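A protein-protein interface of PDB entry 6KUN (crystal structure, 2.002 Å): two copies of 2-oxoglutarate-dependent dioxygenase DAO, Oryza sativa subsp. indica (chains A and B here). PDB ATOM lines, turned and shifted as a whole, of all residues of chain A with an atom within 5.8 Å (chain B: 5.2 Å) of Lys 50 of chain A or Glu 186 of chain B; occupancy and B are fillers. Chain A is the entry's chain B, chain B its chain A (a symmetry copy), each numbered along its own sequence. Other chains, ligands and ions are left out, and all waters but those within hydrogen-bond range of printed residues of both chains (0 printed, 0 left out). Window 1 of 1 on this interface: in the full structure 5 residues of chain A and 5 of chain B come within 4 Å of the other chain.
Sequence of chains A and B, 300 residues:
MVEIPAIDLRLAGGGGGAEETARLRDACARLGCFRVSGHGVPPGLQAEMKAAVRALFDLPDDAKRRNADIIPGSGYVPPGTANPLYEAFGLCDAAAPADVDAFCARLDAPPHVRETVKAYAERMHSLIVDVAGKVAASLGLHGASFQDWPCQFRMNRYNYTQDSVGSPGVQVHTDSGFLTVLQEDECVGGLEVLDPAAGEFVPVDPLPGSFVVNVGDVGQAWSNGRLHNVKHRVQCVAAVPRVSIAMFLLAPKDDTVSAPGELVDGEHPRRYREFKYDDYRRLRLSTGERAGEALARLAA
Of chain B, only Glu 186 comes within 4 Å of Lys 50 of chain A.
Glu 186 of chain B touches just one residue of chain A: Lys 50.
Of the printed residues of chain B, Cys 187 of chain A touches Cys 187.
Printed residues of chain A within 4 Å of Pro 208 of chain B: Arg 54 (3.3 Å).
Of the printed residues of chain B, Arg 54 of chain A touches Pro 208.
Ile 245 of chain A touches none of the printed residues of chain B.
Leu 45 of chain A touches none of the printed residues of chain B.
NZ of Lys 50 of chain A lies within salt-bridge range of OE2 of Glu 186 of chain A, at 3.6 Å.
OD1 of Asp 185 of chain B is in hydrogen-bond range of N of Cys 187 of chain B, 3.1 Å away.
Lys 50 of chain A touches Glu 186 of chain B, but with the chains exchanged Glu 186 of chain A does not touch Lys 50 of chain B (4.4 Å).
Cys 187 of chain B touches its own counterpart, Cys 187 of chain A.
3 positions are printed for both chains.
The side-chain amino group (NZ) of Lys 50 of chain A lies within salt-bridge range of the side-chain carboxylate (OE2) of Glu 186 of chain B (3.3 Å).
The side-chain sulfur (SG) of Cys 187 of chain A forms a disulfide with the side-chain sulfur (SG) of Cys 187 of chain B (2.1 Å).
Among the printed residues, merely in contact across the chains: Arg 54 of chain A with Pro 208 of chain B.
Hydrophobic or aromatic side chains of chain B within 4 Å of the printed part of chain A: Pro 208.
Of the 14 printed residues of chain A, 3 touch a printed residue of chain B.
Among the printed residues, 3 pairs touch across the chains.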
ATOM      1  N   LEU A  45      -8.951  20.706 -33.715  1.00  0.00           N
ATOM      2  CA  LEU A  45     -10.066  20.027 -34.368  1.00  0.00           C
ATOM      3  C   LEU A  45     -11.367  20.296 -33.627  1.00  0.00           C
ATOM      4  O   LEU A  45     -12.402  20.557 -34.239  1.00  0.00           O
ATOM      5  CB  LEU A  45      -9.782  18.512 -34.431  1.00  0.00           C
ATOM      6  CG  LEU A  45     -10.895  17.714 -35.106  1.00  0.00           C
ATOM      7  CD1 LEU A  45     -11.145  18.179 -36.552  1.00  0.00           C
ATOM      8  CD2 LEU A  45     -10.559  16.259 -35.082  1.00  0.00           C
ATOM      9  N   GLN A  46     -11.339  20.264 -32.295  1.00  0.00           N
ATOM     10  CA  GLN A  46     -12.561  20.581 -31.562  1.00  0.00           C
ATOM     11  C   GLN A  46     -13.044  21.984 -31.884  1.00  0.00           C
ATOM     12  O   GLN A  46     -14.255  22.224 -31.966  1.00  0.00           O
ATOM     13  CB  GLN A  46     -12.308  20.451 -30.061  1.00  0.00           C
ATOM     14  CG  GLN A  46     -12.053  19.048 -29.620  1.00  0.00           C
ATOM     15  CD  GLN A  46     -11.766  19.018 -28.166  1.00  0.00           C
ATOM     16  OE1 GLN A  46     -12.587  19.473 -27.372  1.00  0.00           O
ATOM     17  NE2 GLN A  46     -10.589  18.538 -27.799  1.00  0.00           N
ATOM     18  N   ALA A  47     -12.122  22.937 -32.026  1.00  0.00           N
ATOM     19  CA  ALA A  47     -12.530  24.307 -32.334  1.00  0.00           C
ATOM     20  C   ALA A  47     -13.105  24.394 -33.747  1.00  0.00           C
ATOM     21  O   ALA A  47     -14.101  25.080 -34.003  1.00  0.00           O
ATOM     22  CB  ALA A  47     -11.328  25.258 -32.205  1.00  0.00           C
ATOM     23  N   GLU A  48     -12.475  23.724 -34.676  1.00  0.00           N
ATOM     24  CA  GLU A  48     -12.973  23.767 -36.053  1.00  0.00           C
ATOM     25  C   GLU A  48     -14.355  23.118 -36.155  1.00  0.00           C
ATOM     26  O   GLU A  48     -15.214  23.588 -36.921  1.00  0.00           O
ATOM     27  CB  GLU A  48     -11.969  23.066 -36.972  1.00  0.00           C
ATOM     28  CG  GLU A  48     -10.603  23.704 -36.938  1.00  0.00           C
ATOM     29  CD  GLU A  48      -9.557  22.905 -37.672  1.00  0.00           C
ATOM     30  OE1 GLU A  48      -9.921  21.894 -38.306  1.00  0.00           O
ATOM     31  OE2 GLU A  48      -8.368  23.287 -37.604  1.00  0.00           O
ATOM     32  N   MET A  49     -14.592  22.058 -35.375  1.00  0.00           N
ATOM     33  CA  MET A  49     -15.881  21.379 -35.415  1.00  0.00           C
ATOM     34  C   MET A  49     -16.978  22.228 -34.783  1.00  0.00           C
ATOM     35  O   MET A  49     -18.117  22.247 -35.262  1.00  0.00           O
ATOM     36  CB  MET A  49     -15.783  20.037 -34.698  1.00  0.00           C
ATOM     37  CG  MET A  49     -17.068  19.275 -34.685  1.00  0.00           C
ATOM     38  SD  MET A  49     -17.485  18.870 -36.391  1.00  0.00           S
ATOM     39  CE  MET A  49     -18.907  17.817 -36.093  1.00  0.00           C
ATOM     40  N   LYS A  50     -16.672  22.923 -33.687  1.00  0.00           N
ATOM     41  CA  LYS A  50     -17.678  23.802 -33.088  1.00  0.00           C
ATOM     42  C   LYS A  50     -18.178  24.828 -34.100  1.00  0.00           C
ATOM     43  O   LYS A  50     -19.384  25.080 -34.195  1.00  0.00           O
ATOM     44  CB  LYS A  50     -17.087  24.513 -31.854  1.00  0.00           C
ATOM     45  CG  LYS A  50     -18.093  25.360 -31.104  1.00  0.00           C
ATOM     46  CD  LYS A  50     -17.439  26.229 -30.022  1.00  0.00           C
ATOM     47  CE  LYS A  50     -16.824  25.408 -28.893  1.00  0.00           C
ATOM     48  NZ  LYS A  50     -15.809  26.197 -28.127  1.00  0.00           N
ATOM     49  N   ALA A  51     -17.269  25.393 -34.891  1.00  0.00           N
ATOM     50  CA  ALA A  51     -17.649  26.346 -35.932  1.00  0.00           C
ATOM     51  C   ALA A  51     -18.417  25.661 -37.064  1.00  0.00           C
ATOM     52  O   ALA A  51     -19.442  26.167 -37.529  1.00  0.00           O
ATOM     53  CB  ALA A  51     -16.402  27.024 -36.481  1.00  0.00           C
ATOM     54  N   ALA A  52     -17.943  24.502 -37.518  1.00  0.00           N
ATOM     55  CA  ALA A  52     -18.606  23.809 -38.612  1.00  0.00           C
ATOM     56  C   ALA A  52     -20.035  23.426 -38.242  1.00  0.00           C
ATOM     57  O   ALA A  52     -20.962  23.610 -39.038  1.00  0.00           O
ATOM     58  CB  ALA A  52     -17.814  22.552 -39.001  1.00  0.00           C
ATOM     59  N   VAL A  53     -20.240  22.894 -37.040  1.00  0.00           N
ATOM     60  CA  VAL A  53     -21.590  22.510 -36.639  1.00  0.00           C
ATOM     61  C   VAL A  53     -22.503  23.726 -36.575  1.00  0.00           C
ATOM     62  O   VAL A  53     -23.685  23.669 -36.960  1.00  0.00           O
ATOM     63  CB  VAL A  53     -21.550  21.767 -35.297  1.00  0.00           C
ATOM     64  CG1 VAL A  53     -22.964  21.481 -34.824  1.00  0.00           C
ATOM     65  CG2 VAL A  53     -20.809  20.429 -35.461  1.00  0.00           C
ATOM     66  N   ARG A  54     -21.989  24.838 -36.062  1.00  0.00           N
ATOM     67  CA  ARG A  54     -22.776  26.068 -36.059  1.00  0.00           C
ATOM     68  C   ARG A  54     -23.034  26.585 -37.462  1.00  0.00           C
ATOM     69  O   ARG A  54     -24.130  27.081 -37.723  1.00  0.00           O
ATOM     70  CB  ARG A  54     -22.079  27.110 -35.193  1.00  0.00           C
ATOM     71  CG  ARG A  54     -22.555  27.004 -33.728  1.00  0.00           C
ATOM     72  CD  ARG A  54     -21.499  27.321 -32.693  1.00  0.00           C
ATOM     73  NE  ARG A  54     -20.687  28.474 -33.049  1.00  0.00           N
ATOM     74  CZ  ARG A  54     -19.879  29.114 -32.206  1.00  0.00           C
ATOM     75  NH1 ARG A  54     -19.786  28.726 -30.937  1.00  0.00           N
ATOM     76  NH2 ARG A  54     -19.174  30.154 -32.630  1.00  0.00           N
ATOM     77  N   ALA A  55     -22.081  26.399 -38.380  1.00  0.00           N
ATOM     78  CA  ALA A  55     -22.302  26.753 -39.777  1.00  0.00           C
ATOM     79  C   ALA A  55     -23.392  25.887 -40.405  1.00  0.00           C
ATOM     80  O   ALA A  55     -24.271  26.395 -41.110  1.00  0.00           O
ATOM     81  CB  ALA A  55     -20.998  26.614 -40.556  1.00  0.00           C
ATOM     82  N   GLU A 186     -20.260  24.231 -24.538  1.00  0.00           N
ATOM     83  CA  GLU A 186     -19.530  24.803 -23.413  1.00  0.00           C
ATOM     84  C   GLU A 186     -20.337  25.883 -22.702  1.00  0.00           C
ATOM     85  O   GLU A 186     -20.246  26.022 -21.481  1.00  0.00           O
ATOM     86  CB  GLU A 186     -18.207  25.411 -23.890  1.00  0.00           C
ATOM     87  CG  GLU A 186     -17.340  24.498 -24.730  1.00  0.00           C
ATOM     88  CD  GLU A 186     -16.084  25.200 -25.223  1.00  0.00           C
ATOM     89  OE1 GLU A 186     -15.619  24.861 -26.332  1.00  0.00           O
ATOM     90  OE2 GLU A 186     -15.571  26.093 -24.500  1.00  0.00           O
ATOM     91  N   CYS A 187     -21.141  26.636 -23.439  1.00  0.00           N
ATOM     92  CA  CYS A 187     -21.841  27.775 -22.863  1.00  0.00           C
ATOM     93  C   CYS A 187     -23.198  27.423 -22.291  1.00  0.00           C
ATOM     94  O   CYS A 187     -23.614  28.025 -21.300  1.00  0.00           O
ATOM     95  CB  CYS A 187     -21.993  28.857 -23.928  1.00  0.00           C
ATOM     96  SG  CYS A 187     -20.396  29.168 -24.724  1.00  0.00           S
ATOM     97  N   ILE A 245     -22.977  17.418 -29.865  1.00  0.00           N
ATOM     98  CA  ILE A 245     -22.540  16.372 -30.775  1.00  0.00           C
ATOM     99  C   ILE A 245     -22.512  15.078 -29.969  1.00  0.00           C
ATOM    100  O   ILE A 245     -22.024  15.044 -28.817  1.00  0.00           O
ATOM    101  CB  ILE A 245     -21.158  16.704 -31.343  1.00  0.00           C
ATOM    102  CG1 ILE A 245     -21.147  18.113 -31.932  1.00  0.00           C
ATOM    103  CG2 ILE A 245     -20.761  15.750 -32.389  1.00  0.00           C
ATOM    104  CD1 ILE A 245     -19.787  18.607 -32.213  1.00  0.00           C
ATOM    105  N   LYS B  50      -7.878  29.467 -20.868  1.00  0.00           N
ATOM    106  CA  LYS B  50      -9.244  29.557 -20.368  1.00  0.00           C
ATOM    107  C   LYS B  50      -9.384  28.834 -19.035  1.00  0.00           C
ATOM    108  O   LYS B  50      -9.826  29.417 -18.033  1.00  0.00           O
ATOM    109  CB  LYS B  50     -10.202  28.958 -21.406  1.00  0.00           C
ATOM    110  CG  LYS B  50     -11.649  29.365 -21.228  1.00  0.00           C
ATOM    111  CD  LYS B  50     -12.513  28.819 -22.371  1.00  0.00           C
ATOM    112  CE  LYS B  50     -13.606  29.800 -22.804  1.00  0.00           C
ATOM    113  NZ  LYS B  50     -14.867  29.706 -22.006  1.00  0.00           N
ATOM    114  N   GLU B 184     -12.307  37.795 -25.363  1.00  0.00           N
ATOM    115  CA  GLU B 184     -13.579  37.831 -24.650  1.00  0.00           C
ATOM    116  C   GLU B 184     -14.033  36.418 -24.299  1.00  0.00           C
ATOM    117  O   GLU B 184     -13.662  35.439 -24.962  1.00  0.00           O
ATOM    118  CB  GLU B 184     -14.640  38.524 -25.525  1.00  0.00           C
ATOM    119  CG  GLU B 184     -15.885  39.026 -24.795  1.00  0.00           C
ATOM    120  CD  GLU B 184     -16.742  39.935 -25.681  1.00  0.00           C
ATOM    121  OE1 GLU B 184     -16.276  40.299 -26.787  1.00  0.00           O
ATOM    122  OE2 GLU B 184     -17.875  40.283 -25.278  1.00  0.00           O
ATOM    123  N   ASP B 185     -14.823  36.323 -23.230  1.00  0.00           N
ATOM    124  CA  ASP B 185     -15.519  35.082 -22.914  1.00  0.00           C
ATOM    125  C   ASP B 185     -16.354  34.634 -24.106  1.00  0.00           C
ATOM    126  O   ASP B 185     -17.179  35.402 -24.612  1.00  0.00           O
ATOM    127  CB  ASP B 185     -16.434  35.299 -21.711  1.00  0.00           C
ATOM    128  CG  ASP B 185     -16.729  34.024 -20.968  1.00  0.00           C
ATOM    129  OD1 ASP B 185     -16.936  32.966 -21.622  1.00  0.00           O
ATOM    130  OD2 ASP B 185     -16.747  34.089 -19.717  1.00  0.00           O
ATOM    131  N   GLU B 186     -16.142  33.394 -24.563  1.00  0.00           N
ATOM    132  CA  GLU B 186     -16.916  32.868 -25.685  1.00  0.00           C
ATOM    133  C   GLU B 186     -18.409  32.820 -25.375  1.00  0.00           C
ATOM    134  O   GLU B 186     -19.238  33.038 -26.263  1.00  0.00           O
ATOM    135  CB  GLU B 186     -16.398  31.477 -26.042  1.00  0.00           C
ATOM    136  CG  GLU B 186     -14.886  31.435 -26.227  1.00  0.00           C
ATOM    137  CD  GLU B 186     -14.353  30.032 -26.447  1.00  0.00           C
ATOM    138  OE1 GLU B 186     -13.205  29.770 -26.020  1.00  0.00           O
ATOM    139  OE2 GLU B 186     -15.088  29.207 -27.043  1.00  0.00           O
ATOM    140  N   CYS B 187     -18.770  32.591 -24.124  1.00  0.00           N
ATOM    141  CA  CYS B 187     -20.156  32.310 -23.767  1.00  0.00           C
ATOM    142  C   CYS B 187     -20.935  33.519 -23.277  1.00  0.00           C
ATOM    143  O   CYS B 187     -22.163  33.449 -23.196  1.00  0.00           O
ATOM    144  CB  CYS B 187     -20.182  31.282 -22.641  1.00  0.00           C
ATOM    145  SG  CYS B 187     -19.296  29.792 -23.110  1.00  0.00           S
ATOM    146  N   VAL B 188     -20.235  34.603 -22.956  1.00  0.00           N
ATOM    147  CA  VAL B 188     -20.882  35.817 -22.475  1.00  0.00           C
ATOM    148  C   VAL B 188     -20.213  37.054 -23.063  1.00  0.00           C
ATOM    149  O   VAL B 188     -19.208  37.535 -22.541  1.00  0.00           O
ATOM    150  CB  VAL B 188     -20.833  35.908 -20.939  1.00  0.00           C
ATOM    151  CG1 VAL B 188     -21.807  36.962 -20.439  1.00  0.00           C
ATOM    152  CG2 VAL B 188     -21.136  34.553 -20.317  1.00  0.00           C
ATOM    153  N   PRO B 206     -19.088  37.634 -29.331  1.00  0.00           N
ATOM    154  CA  PRO B 206     -17.899  36.776 -29.208  1.00  0.00           C
ATOM    155  C   PRO B 206     -17.747  35.879 -30.429  1.00  0.00           C
ATOM    156  O   PRO B 206     -18.740  35.411 -31.002  1.00  0.00           O
ATOM    157  CB  PRO B 206     -18.173  35.962 -27.935  1.00  0.00           C
ATOM    158  CG  PRO B 206     -19.675  35.918 -27.836  1.00  0.00           C
ATOM    159  CD  PRO B 206     -20.179  37.219 -28.416  1.00  0.00           C
ATOM    160  N   PRO B 208     -15.238  32.600 -31.364  1.00  0.00           N
ATOM    161  CA  PRO B 208     -14.215  31.795 -30.691  1.00  0.00           C
ATOM    162  C   PRO B 208     -12.895  31.783 -31.437  1.00  0.00           C
ATOM    163  O   PRO B 208     -12.860  31.740 -32.665  1.00  0.00           O
ATOM    164  CB  PRO B 208     -14.831  30.389 -30.641  1.00  0.00           C
ATOM    165  CG  PRO B 208     -16.302  30.589 -30.829  1.00  0.00           C
ATOM    166  CD  PRO B 208     -16.436  31.805 -31.704  1.00  0.00           C
